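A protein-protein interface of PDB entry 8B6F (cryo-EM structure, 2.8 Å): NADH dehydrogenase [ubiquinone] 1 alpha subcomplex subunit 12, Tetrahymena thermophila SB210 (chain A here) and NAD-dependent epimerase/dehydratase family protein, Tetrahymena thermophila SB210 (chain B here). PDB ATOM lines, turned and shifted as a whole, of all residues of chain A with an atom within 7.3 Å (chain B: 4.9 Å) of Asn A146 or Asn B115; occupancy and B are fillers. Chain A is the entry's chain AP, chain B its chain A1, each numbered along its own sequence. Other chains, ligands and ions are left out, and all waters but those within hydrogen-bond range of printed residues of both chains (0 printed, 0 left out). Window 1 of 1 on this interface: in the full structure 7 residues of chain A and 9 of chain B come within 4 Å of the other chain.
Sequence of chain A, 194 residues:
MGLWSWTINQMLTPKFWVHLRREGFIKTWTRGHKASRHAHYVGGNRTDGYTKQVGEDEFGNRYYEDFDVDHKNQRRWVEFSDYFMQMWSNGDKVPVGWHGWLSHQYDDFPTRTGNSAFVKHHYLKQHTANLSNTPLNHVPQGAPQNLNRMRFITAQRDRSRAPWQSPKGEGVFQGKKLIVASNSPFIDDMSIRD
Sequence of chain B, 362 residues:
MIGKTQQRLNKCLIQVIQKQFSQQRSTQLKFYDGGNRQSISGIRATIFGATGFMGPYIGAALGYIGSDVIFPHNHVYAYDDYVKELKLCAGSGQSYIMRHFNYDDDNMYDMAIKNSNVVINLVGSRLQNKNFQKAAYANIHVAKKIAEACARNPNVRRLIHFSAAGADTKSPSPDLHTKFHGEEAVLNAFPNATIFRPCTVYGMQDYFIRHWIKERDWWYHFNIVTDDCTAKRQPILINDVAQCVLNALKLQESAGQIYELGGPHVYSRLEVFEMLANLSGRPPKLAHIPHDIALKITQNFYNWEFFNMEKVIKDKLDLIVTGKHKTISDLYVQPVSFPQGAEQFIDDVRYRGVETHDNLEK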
ATOM      1  N   VAL A 139     -26.978  23.055  26.932  1.00  0.00           N
ATOM      2  CA  VAL A 139     -25.600  22.730  26.577  1.00  0.00           C
ATOM      3  C   VAL A 139     -25.453  22.877  25.067  1.00  0.00           C
ATOM      4  O   VAL A 139     -26.052  22.096  24.314  1.00  0.00           O
ATOM      5  CB  VAL A 139     -25.219  21.314  27.034  1.00  0.00           C
ATOM      6  CG1 VAL A 139     -23.789  20.985  26.629  1.00  0.00           C
ATOM      7  CG2 VAL A 139     -25.392  21.174  28.538  1.00  0.00           C
ATOM      8  N   PRO A 140     -24.687  23.850  24.575  1.00  0.00           N
ATOM      9  CA  PRO A 140     -24.522  23.980  23.123  1.00  0.00           C
ATOM     10  C   PRO A 140     -23.927  22.718  22.520  1.00  0.00           C
ATOM     11  O   PRO A 140     -23.070  22.065  23.116  1.00  0.00           O
ATOM     12  CB  PRO A 140     -23.573  25.175  22.978  1.00  0.00           C
ATOM     13  CG  PRO A 140     -23.716  25.936  24.243  1.00  0.00           C
ATOM     14  CD  PRO A 140     -23.988  24.921  25.304  1.00  0.00           C
ATOM     15  N   GLN A 141     -24.398  22.373  21.324  1.00  0.00           N
ATOM     16  CA  GLN A 141     -23.837  21.234  20.611  1.00  0.00           C
ATOM     17  C   GLN A 141     -22.360  21.475  20.338  1.00  0.00           C
ATOM     18  O   GLN A 141     -21.971  22.547  19.866  1.00  0.00           O
ATOM     19  CB  GLN A 141     -24.582  21.010  19.297  1.00  0.00           C
ATOM     20  CG  GLN A 141     -26.071  20.771  19.456  1.00  0.00           C
ATOM     21  CD  GLN A 141     -26.780  20.646  18.126  1.00  0.00           C
ATOM     22  OE1 GLN A 141     -27.843  21.229  17.921  1.00  0.00           O
ATOM     23  NE2 GLN A 141     -26.200  19.876  17.211  1.00  0.00           N
ATOM     24  N   GLY A 142     -21.535  20.478  20.633  1.00  0.00           N
ATOM     25  CA  GLY A 142     -20.107  20.616  20.469  1.00  0.00           C
ATOM     26  C   GLY A 142     -19.393  21.261  21.634  1.00  0.00           C
ATOM     27  O   GLY A 142     -18.158  21.341  21.615  1.00  0.00           O
ATOM     28  N   ALA A 143     -20.122  21.724  22.645  1.00  0.00           N
ATOM     29  CA  ALA A 143     -19.498  22.315  23.811  1.00  0.00           C
ATOM     30  C   ALA A 143     -18.770  21.239  24.612  1.00  0.00           C
ATOM     31  O   ALA A 143     -19.114  20.058  24.541  1.00  0.00           O
ATOM     32  CB  ALA A 143     -20.542  23.005  24.682  1.00  0.00           C
ATOM     33  N   PRO A 144     -17.756  21.624  25.389  1.00  0.00           N
ATOM     34  CA  PRO A 144     -17.008  20.612  26.154  1.00  0.00           C
ATOM     35  C   PRO A 144     -17.880  19.792  27.085  1.00  0.00           C
ATOM     36  O   PRO A 144     -17.593  18.608  27.302  1.00  0.00           O
ATOM     37  CB  PRO A 144     -15.970  21.446  26.922  1.00  0.00           C
ATOM     38  CG  PRO A 144     -16.466  22.851  26.868  1.00  0.00           C
ATOM     39  CD  PRO A 144     -17.207  22.976  25.584  1.00  0.00           C
ATOM     40  N   GLN A 145     -18.936  20.381  27.649  1.00  0.00           N
ATOM     41  CA  GLN A 145     -19.818  19.619  28.526  1.00  0.00           C
ATOM     42  C   GLN A 145     -20.537  18.514  27.764  1.00  0.00           C
ATOM     43  O   GLN A 145     -20.738  17.416  28.295  1.00  0.00           O
ATOM     44  CB  GLN A 145     -20.829  20.547  29.196  1.00  0.00           C
ATOM     45  CG  GLN A 145     -21.779  19.830  30.144  1.00  0.00           C
ATOM     46  CD  GLN A 145     -22.638  20.787  30.944  1.00  0.00           C
ATOM     47  OE1 GLN A 145     -22.408  21.995  30.944  1.00  0.00           O
ATOM     48  NE2 GLN A 145     -23.636  20.248  31.634  1.00  0.00           N
ATOM     49  N   ASN A 146     -20.935  18.783  26.524  1.00  0.00           N
ATOM     50  CA  ASN A 146     -21.643  17.790  25.727  1.00  0.00           C
ATOM     51  C   ASN A 146     -20.715  16.623  25.413  1.00  0.00           C
ATOM     52  O   ASN A 146     -19.718  16.788  24.702  1.00  0.00           O
ATOM     53  CB  ASN A 146     -22.162  18.425  24.441  1.00  0.00           C
ATOM     54  CG  ASN A 146     -23.035  17.486  23.638  1.00  0.00           C
ATOM     55  OD1 ASN A 146     -23.528  16.485  24.154  1.00  0.00           O
ATOM     56  ND2 ASN A 146     -23.232  17.806  22.366  1.00  0.00           N
ATOM     57  N   LEU A 147     -21.045  15.441  25.939  1.00  0.00           N
ATOM     58  CA  LEU A 147     -20.209  14.268  25.719  1.00  0.00           C
ATOM     59  C   LEU A 147     -20.200  13.824  24.263  1.00  0.00           C
ATOM     60  O   LEU A 147     -19.252  13.158  23.839  1.00  0.00           O
ATOM     61  CB  LEU A 147     -20.675  13.117  26.611  1.00  0.00           C
ATOM     62  CG  LEU A 147     -20.641  13.379  28.120  1.00  0.00           C
ATOM     63  CD1 LEU A 147     -21.170  12.175  28.879  1.00  0.00           C
ATOM     64  CD2 LEU A 147     -19.237  13.731  28.592  1.00  0.00           C
ATOM     65  N   ASN A 148     -21.230  14.172  23.492  1.00  0.00           N
ATOM     66  CA  ASN A 148     -21.292  13.857  22.071  1.00  0.00           C
ATOM     67  C   ASN A 148     -20.827  15.026  21.210  1.00  0.00           C
ATOM     68  O   ASN A 148     -21.285  15.187  20.074  1.00  0.00           O
ATOM     69  CB  ASN A 148     -22.709  13.438  21.681  1.00  0.00           C
ATOM     70  CG  ASN A 148     -23.150  12.168  22.373  1.00  0.00           C
ATOM     71  OD1 ASN A 148     -22.329  11.318  22.715  1.00  0.00           O
ATOM     72  ND2 ASN A 148     -24.452  12.029  22.584  1.00  0.00           N
ATOM     73  N   ARG A 149     -19.922  15.852  21.738  1.00  0.00           N
ATOM     74  CA  ARG A 149     -19.407  16.975  20.966  1.00  0.00           C
ATOM     75  C   ARG A 149     -18.650  16.506  19.731  1.00  0.00           C
ATOM     76  O   ARG A 149     -18.549  17.247  18.747  1.00  0.00           O
ATOM     77  CB  ARG A 149     -18.502  17.837  21.845  1.00  0.00           C
ATOM     78  CG  ARG A 149     -17.325  17.081  22.439  1.00  0.00           C
ATOM     79  CD  ARG A 149     -16.447  17.983  23.288  1.00  0.00           C
ATOM     80  NE  ARG A 149     -15.912  19.102  22.524  1.00  0.00           N
ATOM     81  CZ  ARG A 149     -14.951  19.910  22.950  1.00  0.00           C
ATOM     82  NH1 ARG A 149     -14.377  19.741  24.129  1.00  0.00           N
ATOM     83  NH2 ARG A 149     -14.555  20.913  22.173  1.00  0.00           N
ATOM     84  N   MET A 150     -18.110  15.286  19.761  1.00  0.00           N
ATOM     85  CA  MET A 150     -17.318  14.804  18.635  1.00  0.00           C
ATOM     86  C   MET A 150     -18.158  14.703  17.370  1.00  0.00           C
ATOM     87  O   MET A 150     -17.699  15.063  16.281  1.00  0.00           O
ATOM     88  CB  MET A 150     -16.696  13.450  18.973  1.00  0.00           C
ATOM     89  CG  MET A 150     -15.576  13.513  20.002  1.00  0.00           C
ATOM     90  SD  MET A 150     -14.130  14.429  19.428  1.00  0.00           S
ATOM     91  CE  MET A 150     -14.386  16.017  20.217  1.00  0.00           C
ATOM     92  N   ARG A 151     -19.392  14.210  17.492  1.00  0.00           N
ATOM     93  CA  ARG A 151     -20.249  14.082  16.317  1.00  0.00           C
ATOM     94  C   ARG A 151     -20.506  15.441  15.682  1.00  0.00           C
ATOM     95  O   ARG A 151     -20.373  15.606  14.463  1.00  0.00           O
ATOM     96  CB  ARG A 151     -21.566  13.409  16.703  1.00  0.00           C
ATOM     97  CG  ARG A 151     -22.513  13.207  15.534  1.00  0.00           C
ATOM     98  CD  ARG A 151     -23.821  12.574  15.974  1.00  0.00           C
ATOM     99  NE  ARG A 151     -24.699  12.315  14.840  1.00  0.00           N
ATOM    100  CZ  ARG A 151     -25.913  11.790  14.933  1.00  0.00           C
ATOM    101  NH1 ARG A 151     -26.437  11.463  16.103  1.00  0.00           N
ATOM    102  NH2 ARG A 151     -26.619  11.586  13.825  1.00  0.00           N
ATOM    103  N   PHE A 152     -20.879  16.431  16.493  1.00  0.00           N
ATOM    104  CA  PHE A 152     -21.154  17.759  15.957  1.00  0.00           C
ATOM    105  C   PHE A 152     -19.907  18.370  15.331  1.00  0.00           C
ATOM    106  O   PHE A 152     -19.976  18.970  14.252  1.00  0.00           O
ATOM    107  CB  PHE A 152     -21.700  18.662  17.063  1.00  0.00           C
ATOM    108  CG  PHE A 152     -21.967  20.070  16.618  1.00  0.00           C
ATOM    109  CD1 PHE A 152     -23.152  20.395  15.981  1.00  0.00           C
ATOM    110  CD2 PHE A 152     -21.037  21.072  16.848  1.00  0.00           C
ATOM    111  CE1 PHE A 152     -23.402  21.692  15.573  1.00  0.00           C
ATOM    112  CE2 PHE A 152     -21.282  22.370  16.442  1.00  0.00           C
ATOM    113  CZ  PHE A 152     -22.466  22.680  15.806  1.00  0.00           C
ATOM    114  N   ARG B  44      -7.375  18.610  23.449  1.00  0.00           N
ATOM    115  CA  ARG B  44      -8.502  18.482  24.363  1.00  0.00           C
ATOM    116  C   ARG B  44      -7.963  17.833  25.629  1.00  0.00           C
ATOM    117  O   ARG B  44      -7.575  16.661  25.616  1.00  0.00           O
ATOM    118  CB  ARG B  44      -9.629  17.665  23.736  1.00  0.00           C
ATOM    119  CG  ARG B  44     -10.406  18.435  22.680  1.00  0.00           C
ATOM    120  CD  ARG B  44     -11.261  17.534  21.809  1.00  0.00           C
ATOM    121  NE  ARG B  44     -10.477  16.861  20.778  1.00  0.00           N
ATOM    122  CZ  ARG B  44     -10.005  15.624  20.864  1.00  0.00           C
ATOM    123  NH1 ARG B  44     -10.216  14.871  21.931  1.00  0.00           N
ATOM    124  NH2 ARG B  44      -9.303  15.127  19.850  1.00  0.00           N
ATOM    125  N   ILE B 113     -12.750  12.196  30.885  1.00  0.00           N
ATOM    126  CA  ILE B 113     -11.699  12.068  29.881  1.00  0.00           C
ATOM    127  C   ILE B 113     -12.233  11.447  28.590  1.00  0.00           C
ATOM    128  O   ILE B 113     -11.456  10.951  27.779  1.00  0.00           O
ATOM    129  CB  ILE B 113     -10.499  11.270  30.417  1.00  0.00           C
ATOM    130  CG1 ILE B 113     -10.837   9.776  30.468  1.00  0.00           C
ATOM    131  CG2 ILE B 113     -10.095  11.798  31.795  1.00  0.00           C
ATOM    132  CD1 ILE B 113      -9.776   8.917  31.096  1.00  0.00           C
ATOM    133  N   LYS B 114     -13.551  11.465  28.383  1.00  0.00           N
ATOM    134  CA  LYS B 114     -14.109  10.838  27.188  1.00  0.00           C
ATOM    135  C   LYS B 114     -13.581  11.491  25.917  1.00  0.00           C
ATOM    136  O   LYS B 114     -13.205  10.797  24.966  1.00  0.00           O
ATOM    137  CB  LYS B 114     -15.636  10.902  27.226  1.00  0.00           C
ATOM    138  CG  LYS B 114     -16.304  10.384  25.958  1.00  0.00           C
ATOM    139  CD  LYS B 114     -17.812  10.301  26.115  1.00  0.00           C
ATOM    140  CE  LYS B 114     -18.487   9.943  24.799  1.00  0.00           C
ATOM    141  NZ  LYS B 114     -18.000   8.651  24.242  1.00  0.00           N
ATOM    142  N   ASN B 115     -13.541  12.823  25.884  1.00  0.00           N
ATOM    143  CA  ASN B 115     -13.176  13.566  24.685  1.00  0.00           C
ATOM    144  C   ASN B 115     -11.813  14.238  24.804  1.00  0.00           C
ATOM    145  O   ASN B 115     -11.495  15.123  24.004  1.00  0.00           O
ATOM    146  CB  ASN B 115     -14.246  14.611  24.371  1.00  0.00           C
ATOM    147  CG  ASN B 115     -15.574  13.988  24.005  1.00  0.00           C
ATOM    148  OD1 ASN B 115     -15.630  13.040  23.223  1.00  0.00           O
ATOM    149  ND2 ASN B 115     -16.651  14.511  24.578  1.00  0.00           N
ATOM    150  N   SER B 116     -11.001  13.836  25.776  1.00  0.00           N
ATOM    151  CA  SER B 116      -9.707  14.458  26.015  1.00  0.00           C
ATOM    152  C   SER B 116      -8.592  13.551  25.514  1.00  0.00           C
ATOM    153  O   SER B 116      -8.538  12.370  25.872  1.00  0.00           O
ATOM    154  CB  SER B 116      -9.510  14.750  27.503  1.00  0.00           C
ATOM    155  OG  SER B 116     -10.499  15.644  27.978  1.00  0.00           O
ATOM    156  N   ASN B 117      -7.716  14.104  24.679  1.00  0.00           N
ATOM    157  CA  ASN B 117      -6.506  13.411  24.261  1.00  0.00           C
ATOM    158  C   ASN B 117      -5.320  13.700  25.173  1.00  0.00           C
ATOM    159  O   ASN B 117      -4.267  13.076  25.010  1.00  0.00           O
ATOM    160  CB  ASN B 117      -6.152  13.782  22.816  1.00  0.00           C
ATOM    161  CG  ASN B 117      -6.106  15.280  22.588  1.00  0.00           C
ATOM    162  OD1 ASN B 117      -5.953  16.058  23.527  1.00  0.00           O
ATOM    163  ND2 ASN B 117      -6.244  15.690  21.335  1.00  0.00           N
ATOM    164  N   ASN B 153      -9.659   4.371  27.777  1.00  0.00           N
ATOM    165  CA  ASN B 153      -9.983   5.243  26.657  1.00  0.00           C
ATOM    166  C   ASN B 153      -8.850   5.210  25.638  1.00  0.00           C
ATOM    167  O   ASN B 153      -7.725   5.598  25.970  1.00  0.00           O
ATOM    168  CB  ASN B 153     -10.212   6.666  27.140  1.00  0.00           C
ATOM    169  CG  ASN B 153     -10.706   7.583  26.040  1.00  0.00           C
ATOM    170  OD1 ASN B 153     -11.018   7.135  24.938  1.00  0.00           O
ATOM    171  ND2 ASN B 153     -10.788   8.874  26.337  1.00  0.00           N
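The side-chain amide nitrogen (ND2) of Asn B115 sits at hydrogen-bond distance from the backbone carbonyl oxygen (O) of Leu A147, 3.0 Å away.
O of Arg B44 lies close to OD1 of Asn B117, 2.7 Å away.
NE of Arg A149 lies within hydrogen-bond range of O of Gly A142 (3.3 Å).
The backbone NH of Asn A148 lies close to the side-chain amide oxygen of Asn A146, at 3.3 Å.
O of Asn B115 lies within hydrogen-bond range of NH1 of Arg B44 (2.4 Å).
O of Lys B114 lies within hydrogen-bond range of ND2 of Asn B153.
Of chain B, only Asn B115 comes within 4 Å of Asn A146.
Of chain A, only Asn A146, Leu A147, Arg A149 and Met A150 come within 4 Å of Asn B115.
Printed residues of chain A within 4 Å of Arg B44: Met A150 (3.8 Å).
Printed residues of chain B within 4 Å of Met A150: Arg B44 and Asn B115.
Printed residues of chain B within 4 Å of Arg A149: Asn B115.
Of the printed residues of chain A, Lys B114 touches Leu A147.
Printed residues of chain B within 4 Å of Leu A147: Lys B114 (3.4 Å) and Asn B115 (3.0 Å).
The nearest printed residue of chain B that does not touch Arg A149 is Arg B44 (4.4 Å).
Of the 14 printed residues of chain A, 4 touch a printed residue of chain B.
Printed residues of chain A that touch a printed residue of chain B: Asn A146, Leu A147, Arg A149 and Met A150.
Among the printed residues, merely in contact across the chains: Met A150 with Asn B115 (3.3 Å), Arg A149 with Asn B115 (3.4 Å), Leu A147 with Lys B114 (3.4 Å), Met A150 with Arg B44 (3.8 Å) and Asn A146 with Asn B115 (3.8 Å).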
